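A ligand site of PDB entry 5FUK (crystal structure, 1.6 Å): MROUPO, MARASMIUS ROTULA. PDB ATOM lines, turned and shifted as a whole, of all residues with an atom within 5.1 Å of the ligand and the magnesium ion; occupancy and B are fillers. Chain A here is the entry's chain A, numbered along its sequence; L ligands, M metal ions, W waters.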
ATOM      1  N   PRO A  16     -27.541  -1.976 -20.566  1.00  0.00           N
ATOM      2  CA  PRO A  16     -27.367  -2.109 -21.996  1.00  0.00           C
ATOM      3  C   PRO A  16     -28.230  -3.173 -22.691  1.00  0.00           C
ATOM      4  O   PRO A  16     -28.059  -3.410 -23.892  1.00  0.00           O
ATOM      5  CB  PRO A  16     -25.881  -2.522 -22.082  1.00  0.00           C
ATOM      6  CG  PRO A  16     -25.663  -3.401 -20.850  1.00  0.00           C
ATOM      7  CD  PRO A  16     -26.476  -2.685 -19.794  1.00  0.00           C
ATOM      8  N   CYS A  17     -29.095  -3.831 -21.941  1.00  0.00           N
ATOM      9  CA  CYS A  17     -29.898  -4.979 -22.427  1.00  0.00           C
ATOM     10  C   CYS A  17     -31.350  -4.531 -22.628  1.00  0.00           C
ATOM     11  O   CYS A  17     -32.079  -4.255 -21.660  1.00  0.00           O
ATOM     12  CB  CYS A  17     -29.865  -6.100 -21.415  1.00  0.00           C
ATOM     13  SG  CYS A  17     -30.962  -7.460 -21.872  1.00  0.00           S
ATOM     14  N   PRO A  18     -31.813  -4.567 -23.857  1.00  0.00           N
ATOM     15  CA  PRO A  18     -33.203  -4.265 -24.120  1.00  0.00           C
ATOM     16  C   PRO A  18     -34.126  -5.240 -23.519  1.00  0.00           C
ATOM     17  O   PRO A  18     -35.271  -4.904 -23.134  1.00  0.00           O
ATOM     18  CB  PRO A  18     -33.311  -4.286 -25.652  1.00  0.00           C
ATOM     19  CG  PRO A  18     -32.173  -5.140 -26.105  1.00  0.00           C
ATOM     20  CD  PRO A  18     -31.062  -4.864 -25.102  1.00  0.00           C
ATOM     21  N   GLY A  19     -33.707  -6.506 -23.371  1.00  0.00           N
ATOM     22  CA  GLY A  19     -34.600  -7.505 -22.795  1.00  0.00           C
ATOM     23  C   GLY A  19     -34.975  -7.207 -21.364  1.00  0.00           C
ATOM     24  O   GLY A  19     -36.175  -7.211 -20.961  1.00  0.00           O
ATOM     25  N   LEU A  20     -33.952  -6.963 -20.509  1.00  0.00           N
ATOM     26  CA  LEU A  20     -34.193  -6.695 -19.153  1.00  0.00           C
ATOM     27  C   LEU A  20     -34.759  -5.295 -18.966  1.00  0.00           C
ATOM     28  O   LEU A  20     -35.581  -5.108 -18.060  1.00  0.00           O
ATOM     29  CB  LEU A  20     -32.900  -6.833 -18.338  1.00  0.00           C
ATOM     30  CG  LEU A  20     -32.225  -8.201 -18.424  1.00  0.00           C
ATOM     31  CD1 LEU A  20     -30.913  -8.182 -17.619  1.00  0.00           C
ATOM     32  CD2 LEU A  20     -33.128  -9.247 -17.835  1.00  0.00           C
ATOM     33  N   LEU A  23     -38.497  -5.553 -19.499  1.00  0.00           N
ATOM     34  CA  LEU A  23     -39.159  -6.200 -18.372  1.00  0.00           C
ATOM     35  C   LEU A  23     -39.315  -5.211 -17.240  1.00  0.00           C
ATOM     36  O   LEU A  23     -40.336  -5.210 -16.592  1.00  0.00           O
ATOM     37  CB  LEU A  23     -38.400  -7.419 -17.892  1.00  0.00           C
ATOM     38  CG  LEU A  23     -38.443  -8.572 -18.918  1.00  0.00           C
ATOM     39  CD1 LEU A  23     -37.476  -9.689 -18.485  1.00  0.00           C
ATOM     40  CD2 LEU A  23     -39.834  -9.182 -19.097  1.00  0.00           C
ATOM     41  N   ILE A  41     -34.998 -12.527 -12.225  1.00  0.00           N
ATOM     42  CA  ILE A  41     -34.820 -12.559 -13.709  1.00  0.00           C
ATOM     43  C   ILE A  41     -35.516 -13.750 -14.273  1.00  0.00           C
ATOM     44  O   ILE A  41     -36.181 -13.629 -15.284  1.00  0.00           O
ATOM     45  CB  ILE A  41     -33.330 -12.469 -14.110  1.00  0.00           C
ATOM     46  CG1 ILE A  41     -32.707 -11.113 -13.717  1.00  0.00           C
ATOM     47  CG2 ILE A  41     -33.143 -12.765 -15.572  1.00  0.00           C
ATOM     48  CD1 ILE A  41     -31.167 -11.020 -13.834  1.00  0.00           C
ATOM     49  N   GLY A  45     -38.522 -13.214 -16.891  1.00  0.00           N
ATOM     50  CA  GLY A  45     -38.367 -13.686 -18.285  1.00  0.00           C
ATOM     51  C   GLY A  45     -39.427 -14.673 -18.654  1.00  0.00           C
ATOM     52  O   GLY A  45     -39.895 -14.724 -19.757  1.00  0.00           O
ATOM     53  N   TYR A  49     -41.905 -13.089 -21.438  1.00  0.00           N
ATOM     54  CA  TYR A  49     -41.490 -13.561 -22.732  1.00  0.00           C
ATOM     55  C   TYR A  49     -41.609 -15.067 -22.991  1.00  0.00           C
ATOM     56  O   TYR A  49     -41.381 -15.494 -24.142  1.00  0.00           O
ATOM     57  CB  TYR A  49     -39.986 -13.220 -22.921  1.00  0.00           C
ATOM     58  CG  TYR A  49     -39.549 -11.754 -22.797  1.00  0.00           C
ATOM     59  CD1 TYR A  49     -40.289 -10.701 -23.365  1.00  0.00           C
ATOM     60  CD2 TYR A  49     -38.326 -11.449 -22.193  1.00  0.00           C
ATOM     61  CE1 TYR A  49     -39.847  -9.395 -23.303  1.00  0.00           C
ATOM     62  CE2 TYR A  49     -37.871 -10.157 -22.107  1.00  0.00           C
ATOM     63  CZ  TYR A  49     -38.622  -9.118 -22.658  1.00  0.00           C
ATOM     64  OH  TYR A  49     -38.223  -7.831 -22.621  1.00  0.00           O
ATOM     65  N   VAL A  51     -39.467 -17.114 -21.790  1.00  0.00           N
ATOM     66  CA  VAL A  51     -38.094 -17.589 -21.790  1.00  0.00           C
ATOM     67  C   VAL A  51     -37.862 -18.379 -20.509  1.00  0.00           C
ATOM     68  O   VAL A  51     -38.249 -17.961 -19.387  1.00  0.00           O
ATOM     69  CB  VAL A  51     -37.083 -16.401 -21.843  1.00  0.00           C
ATOM     70  CG1 VAL A  51     -35.666 -16.900 -21.683  1.00  0.00           C
ATOM     71  CG2 VAL A  51     -37.197 -15.681 -23.171  1.00  0.00           C
ATOM     72  N   LEU A  56     -31.672 -18.193 -18.637  1.00  0.00           N
ATOM     73  CA  LEU A  56     -31.670 -17.045 -17.730  1.00  0.00           C
ATOM     74  C   LEU A  56     -30.789 -17.278 -16.499  1.00  0.00           C
ATOM     75  O   LEU A  56     -30.245 -16.352 -15.959  1.00  0.00           O
ATOM     76  CB  LEU A  56     -33.098 -16.736 -17.300  1.00  0.00           C
ATOM     77  CG  LEU A  56     -33.953 -16.212 -18.481  1.00  0.00           C
ATOM     78  CD1 LEU A  56     -35.305 -16.062 -17.956  1.00  0.00           C
ATOM     79  CD2 LEU A  56     -33.395 -14.966 -19.135  1.00  0.00           C
ATOM     80  N   ALA A  59     -27.023 -16.934 -18.053  1.00  0.00           N
ATOM     81  CA  ALA A  59     -26.668 -15.550 -18.298  1.00  0.00           C
ATOM     82  C   ALA A  59     -26.767 -14.702 -17.040  1.00  0.00           C
ATOM     83  O   ALA A  59     -25.912 -13.852 -16.794  1.00  0.00           O
ATOM     84  CB  ALA A  59     -27.593 -14.954 -19.371  1.00  0.00           C
ATOM     85  N   GLY A  60     -27.770 -14.957 -16.256  1.00  0.00           N
ATOM     86  CA  GLY A  60     -28.009 -14.223 -15.009  1.00  0.00           C
ATOM     87  C   GLY A  60     -26.871 -14.303 -14.027  1.00  0.00           C
ATOM     88  O   GLY A  60     -26.437 -13.267 -13.490  1.00  0.00           O
ATOM     89  N   GLY A  63     -24.050 -12.219 -15.182  1.00  0.00           N
ATOM     90  CA  GLY A  63     -24.407 -10.804 -14.938  1.00  0.00           C
ATOM     91  C   GLY A  63     -24.251 -10.381 -13.484  1.00  0.00           C
ATOM     92  O   GLY A  63     -23.829  -9.222 -13.210  1.00  0.00           O
ATOM     93  N   ILE A  73     -27.996  -7.281  -8.547  1.00  0.00           N
ATOM     94  CA  ILE A  73     -27.448  -6.190  -9.370  1.00  0.00           C
ATOM     95  C   ILE A  73     -28.472  -5.072  -9.475  1.00  0.00           C
ATOM     96  O   ILE A  73     -29.667  -5.263  -9.235  1.00  0.00           O
ATOM     97  CB  ILE A  73     -27.141  -6.636 -10.826  1.00  0.00           C
ATOM     98  CG1 ILE A  73     -28.407  -7.092 -11.526  1.00  0.00           C
ATOM     99  CG2 ILE A  73     -26.054  -7.741 -10.867  1.00  0.00           C
ATOM    100  CD1 ILE A  73     -28.172  -7.384 -13.014  1.00  0.00           C
ATOM    101  N   LEU A  78     -24.691  -3.926 -15.453  1.00  0.00           N
ATOM    102  CA  LEU A  78     -24.433  -4.782 -16.614  1.00  0.00           C
ATOM    103  C   LEU A  78     -23.676  -4.103 -17.738  1.00  0.00           C
ATOM    104  O   LEU A  78     -23.171  -4.785 -18.652  1.00  0.00           O
ATOM    105  CB  LEU A  78     -25.751  -5.308 -17.151  1.00  0.00           C
ATOM    106  CG  LEU A  78     -26.530  -6.248 -16.264  1.00  0.00           C
ATOM    107  CD1 LEU A  78     -27.937  -6.607 -16.736  1.00  0.00           C
ATOM    108  CD2 LEU A  78     -25.767  -7.578 -15.990  1.00  0.00           C
ATOM    109  N   ILE A  84     -20.233  -9.327 -19.732  1.00  0.00           N
ATOM    110  CA  ILE A  84     -21.086  -9.616 -20.883  1.00  0.00           C
ATOM    111  C   ILE A  84     -21.004  -8.524 -21.956  1.00  0.00           C
ATOM    112  O   ILE A  84     -20.880  -8.790 -23.098  1.00  0.00           O
ATOM    113  CB  ILE A  84     -22.542  -9.857 -20.478  1.00  0.00           C
ATOM    114  CG1 ILE A  84     -22.624 -11.045 -19.559  1.00  0.00           C
ATOM    115  CG2 ILE A  84     -23.413 -10.110 -21.699  1.00  0.00           C
ATOM    116  CD1 ILE A  84     -23.962 -11.217 -18.928  1.00  0.00           C
ATOM    117  N   GLU A  85     -21.054  -7.290 -21.523  1.00  0.00           N
ATOM    118  CA  GLU A  85     -21.050  -6.180 -22.457  1.00  0.00           C
ATOM    119  C   GLU A  85     -19.871  -6.263 -23.328  1.00  0.00           C
ATOM    120  O   GLU A  85     -18.733  -6.506 -22.896  1.00  0.00           O
ATOM    121  CB  GLU A  85     -21.091  -4.858 -21.742  1.00  0.00           C
ATOM    122  CG  GLU A  85     -21.540  -3.688 -22.636  1.00  0.00           C
ATOM    123  CD  GLU A  85     -20.394  -3.145 -23.417  1.00  0.00           C
ATOM    124  OE1 GLU A  85     -19.249  -3.061 -22.926  1.00  0.00           O
ATOM    125  OE2 GLU A  85     -20.549  -2.848 -24.623  1.00  0.00           O
ATOM    126  N   HIS A  86     -20.093  -5.993 -24.603  1.00  0.00           N
ATOM    127  CA  HIS A  86     -19.093  -6.226 -25.641  1.00  0.00           C
ATOM    128  C   HIS A  86     -19.192  -5.177 -26.755  1.00  0.00           C
ATOM    129  O   HIS A  86     -20.210  -4.470 -26.948  1.00  0.00           O
ATOM    130  CB  HIS A  86     -19.296  -7.590 -26.311  1.00  0.00           C
ATOM    131  CG  HIS A  86     -20.670  -7.774 -26.797  1.00  0.00           C
ATOM    132  ND1 HIS A  86     -21.149  -7.201 -27.936  1.00  0.00           N
ATOM    133  CD2 HIS A  86     -21.704  -8.432 -26.258  1.00  0.00           C
ATOM    134  CE1 HIS A  86     -22.430  -7.479 -28.078  1.00  0.00           C
ATOM    135  NE2 HIS A  86     -22.792  -8.248 -27.066  1.00  0.00           N
ATOM    136  N   ASP A  87     -18.096  -5.052 -27.499  1.00  0.00           N
ATOM    137  CA  ASP A  87     -18.113  -4.190 -28.675  1.00  0.00           C
ATOM    138  C   ASP A  87     -18.974  -4.803 -29.807  1.00  0.00           C
ATOM    139  O   ASP A  87     -19.377  -5.977 -29.725  1.00  0.00           O
ATOM    140  CB  ASP A  87     -16.709  -4.058 -29.212  1.00  0.00           C
ATOM    141  CG  ASP A  87     -15.747  -3.484 -28.188  1.00  0.00           C
ATOM    142  OD1 ASP A  87     -16.123  -2.595 -27.450  1.00  0.00           O
ATOM    143  OD2 ASP A  87     -14.541  -3.845 -28.260  1.00  0.00           O
ATOM    144  N   SER A  89     -22.050  -4.053 -30.617  1.00  0.00           N
ATOM    145  CA  SER A  89     -23.461  -4.158 -30.223  1.00  0.00           C
ATOM    146  C   SER A  89     -24.319  -3.661 -31.392  1.00  0.00           C
ATOM    147  O   SER A  89     -23.862  -2.927 -32.322  1.00  0.00           O
ATOM    148  CB  SER A  89     -23.771  -3.345 -28.964  1.00  0.00           C
ATOM    149  OG  SER A  89     -23.079  -3.866 -27.839  1.00  0.00           O
ATOM    150  N   LEU A  90     -25.575  -4.123 -31.356  1.00  0.00           N
ATOM    151  CA  LEU A  90     -26.549  -3.788 -32.386  1.00  0.00           C
ATOM    152  C   LEU A  90     -27.126  -2.369 -32.179  1.00  0.00           C
ATOM    153  O   LEU A  90     -27.600  -1.757 -33.168  1.00  0.00           O
ATOM    154  CB  LEU A  90     -27.720  -4.727 -32.267  1.00  0.00           C
ATOM    155  CG  LEU A  90     -27.394  -6.216 -32.552  1.00  0.00           C
ATOM    156  CD1 LEU A  90     -28.534  -7.118 -32.045  1.00  0.00           C
ATOM    157  CD2 LEU A  90     -27.109  -6.475 -33.999  1.00  0.00           C
ATOM    158  N   SER A  91     -26.987  -1.816 -30.973  1.00  0.00           N
ATOM    159  CA  SER A  91     -27.703  -0.557 -30.721  1.00  0.00           C
ATOM    160  C   SER A  91     -26.992   0.378 -29.768  1.00  0.00           C
ATOM    161  O   SER A  91     -27.550   1.426 -29.421  1.00  0.00           O
ATOM    162  CB  SER A  91     -29.122  -0.790 -30.174  1.00  0.00           C
ATOM    163  OG  SER A  91     -29.132  -1.369 -28.855  1.00  0.00           O
ATOM    164  N   ARG A  92     -25.806  -0.040 -29.343  1.00  0.00           N
ATOM    165  CA  ARG A  92     -24.962   0.765 -28.443  1.00  0.00           C
ATOM    166  C   ARG A  92     -23.633   0.941 -29.160  1.00  0.00           C
ATOM    167  O   ARG A  92     -23.125   0.179 -30.022  1.00  0.00           O
ATOM    168  CB  ARG A  92     -24.726   0.082 -27.092  1.00  0.00           C
ATOM    169  CG  ARG A  92     -25.722   0.299 -26.017  1.00  0.00           C
ATOM    170  CD  ARG A  92     -27.196  -0.070 -26.320  1.00  0.00           C
ATOM    171  NE  ARG A  92     -28.035   0.072 -25.178  1.00  0.00           N
ATOM    172  CZ  ARG A  92     -29.347  -0.131 -25.139  1.00  0.00           C
ATOM    173  NH1 ARG A  92     -29.979  -0.536 -26.260  1.00  0.00           N
ATOM    174  NH2 ARG A  92     -30.036   0.100 -24.041  1.00  0.00           N
ATOM    175  N   GLU A  93     -22.943   2.000 -28.689  1.00  0.00           N
ATOM    176  CA  GLU A  93     -21.562   2.213 -29.152  1.00  0.00           C
ATOM    177  C   GLU A  93     -20.533   1.399 -28.368  1.00  0.00           C
ATOM    178  O   GLU A  93     -20.785   1.052 -27.201  1.00  0.00           O
ATOM    179  CB  GLU A  93     -21.194   3.738 -29.026  1.00  0.00           C
ATOM    180  CG  GLU A  93     -22.102   4.614 -29.819  1.00  0.00           C
ATOM    181  CD  GLU A  93     -21.870   6.147 -29.562  1.00  0.00           C
ATOM    182  OE1 GLU A  93     -21.682   6.610 -28.403  1.00  0.00           O
ATOM    183  OE2 GLU A  93     -21.969   6.901 -30.567  1.00  0.00           O
ATOM    184  N   ASN A 100     -21.541   2.949 -24.191  1.00  0.00           N
ATOM    185  CA  ASN A 100     -21.877   1.504 -24.318  1.00  0.00           C
ATOM    186  C   ASN A 100     -23.125   1.137 -23.542  1.00  0.00           C
ATOM    187  O   ASN A 100     -23.465  -0.055 -23.444  1.00  0.00           O
ATOM    188  CB  ASN A 100     -20.711   0.651 -23.845  1.00  0.00           C
ATOM    189  CG  ASN A 100     -20.585   0.650 -22.303  1.00  0.00           C
ATOM    190  OD1 ASN A 100     -21.129   1.533 -21.591  1.00  0.00           O
ATOM    191  ND2 ASN A 100     -19.958  -0.409 -21.756  1.00  0.00           N
ATOM    192  N   GLU A 157     -27.637 -12.934 -28.584  1.00  0.00           N
ATOM    193  CA  GLU A 157     -28.479 -11.748 -28.460  1.00  0.00           C
ATOM    194  C   GLU A 157     -29.360 -11.576 -29.708  1.00  0.00           C
ATOM    195  O   GLU A 157     -30.550 -11.271 -29.597  1.00  0.00           O
ATOM    196  CB  GLU A 157     -27.598 -10.530 -28.161  1.00  0.00           C
ATOM    197  CG  GLU A 157     -27.102 -10.621 -26.707  1.00  0.00           C
ATOM    198  CD  GLU A 157     -25.858  -9.811 -26.352  1.00  0.00           C
ATOM    199  OE1 GLU A 157     -25.281  -9.215 -27.248  1.00  0.00           O
ATOM    200  OE2 GLU A 157     -25.409  -9.888 -25.139  1.00  0.00           O
ATOM    201  N   PHE A 160     -32.095 -14.009 -29.374  1.00  0.00           N
ATOM    202  CA  PHE A 160     -33.045 -13.547 -28.382  1.00  0.00           C
ATOM    203  C   PHE A 160     -34.102 -12.587 -28.964  1.00  0.00           C
ATOM    204  O   PHE A 160     -35.296 -12.713 -28.661  1.00  0.00           O
ATOM    205  CB  PHE A 160     -32.323 -12.854 -27.208  1.00  0.00           C
ATOM    206  CG  PHE A 160     -32.282 -13.631 -25.897  1.00  0.00           C
ATOM    207  CD1 PHE A 160     -33.297 -14.535 -25.527  1.00  0.00           C
ATOM    208  CD2 PHE A 160     -31.237 -13.376 -25.006  1.00  0.00           C
ATOM    209  CE1 PHE A 160     -33.247 -15.202 -24.300  1.00  0.00           C
ATOM    210  CE2 PHE A 160     -31.177 -14.016 -23.768  1.00  0.00           C
ATOM    211  CZ  PHE A 160     -32.190 -14.937 -23.417  1.00  0.00           C
ATOM    212  N   PHE A 161     -33.683 -11.610 -29.756  1.00  0.00           N
ATOM    213  CA  PHE A 161     -34.660 -10.658 -30.307  1.00  0.00           C
ATOM    214  C   PHE A 161     -35.533 -11.333 -31.332  1.00  0.00           C
ATOM    215  O   PHE A 161     -36.750 -11.122 -31.360  1.00  0.00           O
ATOM    216  CB  PHE A 161     -34.099  -9.307 -30.715  1.00  0.00           C
ATOM    217  CG  PHE A 161     -33.496  -9.234 -32.061  1.00  0.00           C
ATOM    218  CD1 PHE A 161     -34.265  -9.301 -33.244  1.00  0.00           C
ATOM    219  CD2 PHE A 161     -32.127  -9.048 -32.193  1.00  0.00           C
ATOM    220  CE1 PHE A 161     -33.650  -9.284 -34.518  1.00  0.00           C
ATOM    221  CE2 PHE A 161     -31.536  -8.987 -33.444  1.00  0.00           C
ATOM    222  CZ  PHE A 161     -32.315  -9.068 -34.610  1.00  0.00           C
ATOM    223  N   VAL A 164     -37.995 -13.831 -29.095  1.00  0.00           N
ATOM    224  CA  VAL A 164     -38.860 -13.242 -28.156  1.00  0.00           C
ATOM    225  C   VAL A 164     -39.859 -12.283 -28.844  1.00  0.00           C
ATOM    226  O   VAL A 164     -40.974 -12.143 -28.342  1.00  0.00           O
ATOM    227  CB  VAL A 164     -38.051 -12.488 -27.042  1.00  0.00           C
ATOM    228  CG1 VAL A 164     -38.881 -11.626 -26.216  1.00  0.00           C
ATOM    229  CG2 VAL A 164     -37.328 -13.483 -26.180  1.00  0.00           C
ATOM    230  N   PHE A 183     -39.126  -2.607 -29.588  1.00  0.00           N
ATOM    231  CA  PHE A 183     -38.377  -3.254 -28.483  1.00  0.00           C
ATOM    232  C   PHE A 183     -37.046  -2.526 -28.287  1.00  0.00           C
ATOM    233  O   PHE A 183     -36.719  -2.192 -27.160  1.00  0.00           O
ATOM    234  CB  PHE A 183     -38.140  -4.710 -28.908  1.00  0.00           C
ATOM    235  CG  PHE A 183     -37.339  -5.549 -27.941  1.00  0.00           C
ATOM    236  CD1 PHE A 183     -37.807  -5.797 -26.680  1.00  0.00           C
ATOM    237  CD2 PHE A 183     -36.134  -6.115 -28.349  1.00  0.00           C
ATOM    238  CE1 PHE A 183     -37.073  -6.620 -25.830  1.00  0.00           C
ATOM    239  CE2 PHE A 183     -35.390  -6.912 -27.489  1.00  0.00           C
ATOM    240  CZ  PHE A 183     -35.877  -7.163 -26.259  1.00  0.00           C
ATOM    241  N   PHE A 184     -36.256  -2.297 -29.344  1.00  0.00           N
ATOM    242  CA  PHE A 184     -34.985  -1.588 -29.159  1.00  0.00           C
ATOM    243  C   PHE A 184     -35.185  -0.090 -28.842  1.00  0.00           C
ATOM    244  O   PHE A 184     -34.573   0.431 -27.931  1.00  0.00           O
ATOM    245  CB  PHE A 184     -34.102  -1.743 -30.368  1.00  0.00           C
ATOM    246  CG  PHE A 184     -33.320  -3.031 -30.409  1.00  0.00           C
ATOM    247  CD1 PHE A 184     -32.065  -3.092 -29.832  1.00  0.00           C
ATOM    248  CD2 PHE A 184     -33.777  -4.106 -31.082  1.00  0.00           C
ATOM    249  CE1 PHE A 184     -31.342  -4.273 -29.972  1.00  0.00           C
ATOM    250  CE2 PHE A 184     -33.050  -5.304 -31.186  1.00  0.00           C
ATOM    251  CZ  PHE A 184     -31.828  -5.358 -30.623  1.00  0.00           C
HETATM  252  C1  LIG L   1     -27.690  -7.297 -24.661  1.00  0.00           C
HETATM  253  C2  LIG L   1     -31.945  -9.375 -25.302  1.00  0.00           C
HETATM  254  C3  LIG L   1     -31.550 -11.358 -20.902  1.00  0.00           C
HETATM  255  C4  LIG L   1     -27.391  -9.044 -20.220  1.00  0.00           C
HETATM  256  C5  LIG L   1     -28.839  -7.768 -25.262  1.00  0.00           C
HETATM  257  C6  LIG L   1     -29.164  -7.559 -26.629  1.00  0.00           C
HETATM  258  C7  LIG L   1     -30.410  -8.145 -26.805  1.00  0.00           C
HETATM  259  C8  LIG L   1     -30.776  -8.719 -25.594  1.00  0.00           C
HETATM  260  C9  LIG L   1     -31.220  -8.226 -28.055  1.00  0.00           C
HETATM  261  C10 LIG L   1     -28.374  -6.868 -27.674  1.00  0.00           C
HETATM  262  C11 LIG L   1     -28.345  -5.329 -27.555  1.00  0.00           C
HETATM  263  C12 LIG L   1     -27.344  -4.747 -28.577  1.00  0.00           C
HETATM  264  O1  LIG L   1     -27.386  -3.508 -28.806  1.00  0.00           O
HETATM  265  O2  LIG L   1     -26.504  -5.416 -29.185  1.00  0.00           O
HETATM  266  C13 LIG L   1     -32.239 -10.068 -24.143  1.00  0.00           C
HETATM  267  C14 LIG L   1     -33.478 -10.763 -23.916  1.00  0.00           C
HETATM  268  C15 LIG L   1     -33.372 -11.362 -22.709  1.00  0.00           C
HETATM  269  C16 LIG L   1     -32.055 -10.953 -22.136  1.00  0.00           C
HETATM  270  C17 LIG L   1     -34.667 -10.916 -24.897  1.00  0.00           C
HETATM  271  C18 LIG L   1     -34.436 -12.171 -22.080  1.00  0.00           C
HETATM  272  C19 LIG L   1     -34.724 -12.051 -20.796  1.00  0.00           C
HETATM  273  C20 LIG L   1     -30.331 -10.998 -20.372  1.00  0.00           C
HETATM  274  C21 LIG L   1     -29.822 -11.435 -19.087  1.00  0.00           C
HETATM  275  C22 LIG L   1     -28.661 -10.756 -18.925  1.00  0.00           C
HETATM  276  C23 LIG L   1     -28.436  -9.913 -20.052  1.00  0.00           C
HETATM  277  C24 LIG L   1     -30.493 -12.460 -18.230  1.00  0.00           C
HETATM  278  C25 LIG L   1     -27.752 -10.744 -17.762  1.00  0.00           C
HETATM  279  C26 LIG L   1     -28.176 -10.816 -16.471  1.00  0.00           C
HETATM  280  C27 LIG L   1     -27.183  -8.324 -21.367  1.00  0.00           C
HETATM  281  C28 LIG L   1     -25.995  -7.472 -21.539  1.00  0.00           C
HETATM  282  C29 LIG L   1     -26.101  -6.931 -22.772  1.00  0.00           C
HETATM  283  C30 LIG L   1     -27.290  -7.546 -23.377  1.00  0.00           C
HETATM  284  C31 LIG L   1     -24.953  -7.159 -20.510  1.00  0.00           C
HETATM  285  C32 LIG L   1     -25.134  -6.037 -23.494  1.00  0.00           C
HETATM  286  C33 LIG L   1     -24.255  -6.734 -24.517  1.00  0.00           C
HETATM  287  C34 LIG L   1     -23.804  -5.722 -25.562  1.00  0.00           C
HETATM  288  O3  LIG L   1     -22.672  -5.176 -25.412  1.00  0.00           O
HETATM  289  O4  LIG L   1     -24.546  -5.453 -26.530  1.00  0.00           O
HETATM  290  N1  LIG L   1     -29.836  -8.480 -24.597  1.00  0.00           N
HETATM  291  N2  LIG L   1     -31.441 -10.202 -23.055  1.00  0.00           N
HETATM  292  N3  LIG L   1     -29.472 -10.079 -20.914  1.00  0.00           N
HETATM  293  N4  LIG L   1     -27.933  -8.326 -22.501  1.00  0.00           N
HETATM  294 FE1  LIG L   1     -29.678  -9.230 -22.758  1.00  0.00          FE
HETATM  295 MG    MG M   1     -21.904  -3.350 -26.194  1.00  0.00          MG
HETATM  296  O   HOH W   1     -23.416  -2.244 -25.205  1.00  0.00           O
HETATM  297  O   HOH W   2     -21.168  -1.722 -27.273  1.00  0.00           O
HETATM  298  O   HOH W   3     -25.974  -3.048 -25.669  1.00  0.00           O
HETATM  299  O   HOH W   4     -25.257  -7.830 -29.607  1.00  0.00           O
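The backbone NH (N) of His 86 lies close to an oxygen (O3) of the ligand. An oxygen (O4) of the ligand lies close to a ring nitrogen (NE2) of His 86, at 3.3 Å. The side-chain sulfur of Cys 17 binds an iron atom (FE1) of the ligand (2.4 Å). The backbone NH of Leu 90 is in hydrogen-bond range of an oxygen (O2) of the ligand, at 2.7 Å. O1 of the ligand sits at hydrogen-bond distance from N of Ser 91 (2.8 Å). An oxygen (O1) of the ligand sits at hydrogen-bond distance from the side-chain hydroxyl of Ser 91 (2.8 Å).
The side-chain carboxylate of Glu 85 is in hydrogen-bond range of the side-chain amide nitrogen of Asn 100. A ring nitrogen (NE2) of His 86 is in hydrogen-bond range of the side-chain carboxylate (OE1) of Glu 157, 2.7 Å away. The backbone NH (N) of Gly 19 lies close to the side-chain sulfur (SG) of Cys 17 (3.3 Å). SG of Cys 17 sits close to N of Leu 20 (3.3 Å). OG of Ser 91 lies within hydrogen-bond range of NH1 of Arg 92 (2.9 Å). OH of Tyr 49 is in hydrogen-bond range of O of Gly 19 (2.7 Å).
CG of Pro 16 touches C32 of the ligand (3.8 Å). Pro 18 touches the ligand (CG to C7, 3.6 Å). Gly 19 touches the ligand (CA to C14, 3.6 Å). Leu 20 touches the ligand. Ile 41 touches the ligand (CG2 to C24, 3.8 Å). CE2 of Tyr 49 touches C19 of the ligand, 3.9 Å away. CD2 of Leu 56 touches C19 of the ligand, at 3.6 Å. O of Ala 59 touches C25 of the ligand (3.7 Å). CA of Gly 60 touches C26 of the ligand (3.7 Å). Leu 78 touches the ligand. Ile 84 touches the ligand. Arg 92 touches the ligand. Glu 157 touches the ligand (OE2 to C33, 3.4 Å). CD2 of Phe 160 touches C13 of the ligand, at 3.6 Å. Val 164 touches the ligand. Phe 184 touches the ligand. Hydrophobic or aromatic side chains within 4 Å of the ligand: Pro 16, Pro 18, Leu 20, Ile 41, Tyr 49, Leu 56, Ala 59, Leu 78, Ile 84, His 86, Leu 90, Phe 160, Val 164 and Phe 184. Of the 32 residues printed, 22 come within 4 Å of the ligand. The nearest printed residue that does not touch the ligand is Phe 161 (4.1 Å).
Of the 32 residues printed, 3 come within 4 Å of the magnesium ion.
The magnesium ion is bound by the side-chain hydroxyl (OG) of Ser 89 (2.1 Å), water W2 (2.1 Å), water W1 (2.1 Å), an oxygen (O3) of the ligand (2.1 Å), the side-chain carboxylate (OE2) of Glu 85 (2.1 Å) and the backbone carbonyl oxygen (O) of His 86 (2.2 Å). The magnesium ion has six donor atoms within binding distance.
Water W4 bridges the side-chain carboxylate of Glu 157 (2.7 Å) and an oxygen (O2) of the ligand (2.7 Å). Water W3 bridges the backbone carbonyl oxygen of Pro 16 (2.8 Å) and an oxygen (O4) of the ligand (2.9 Å).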
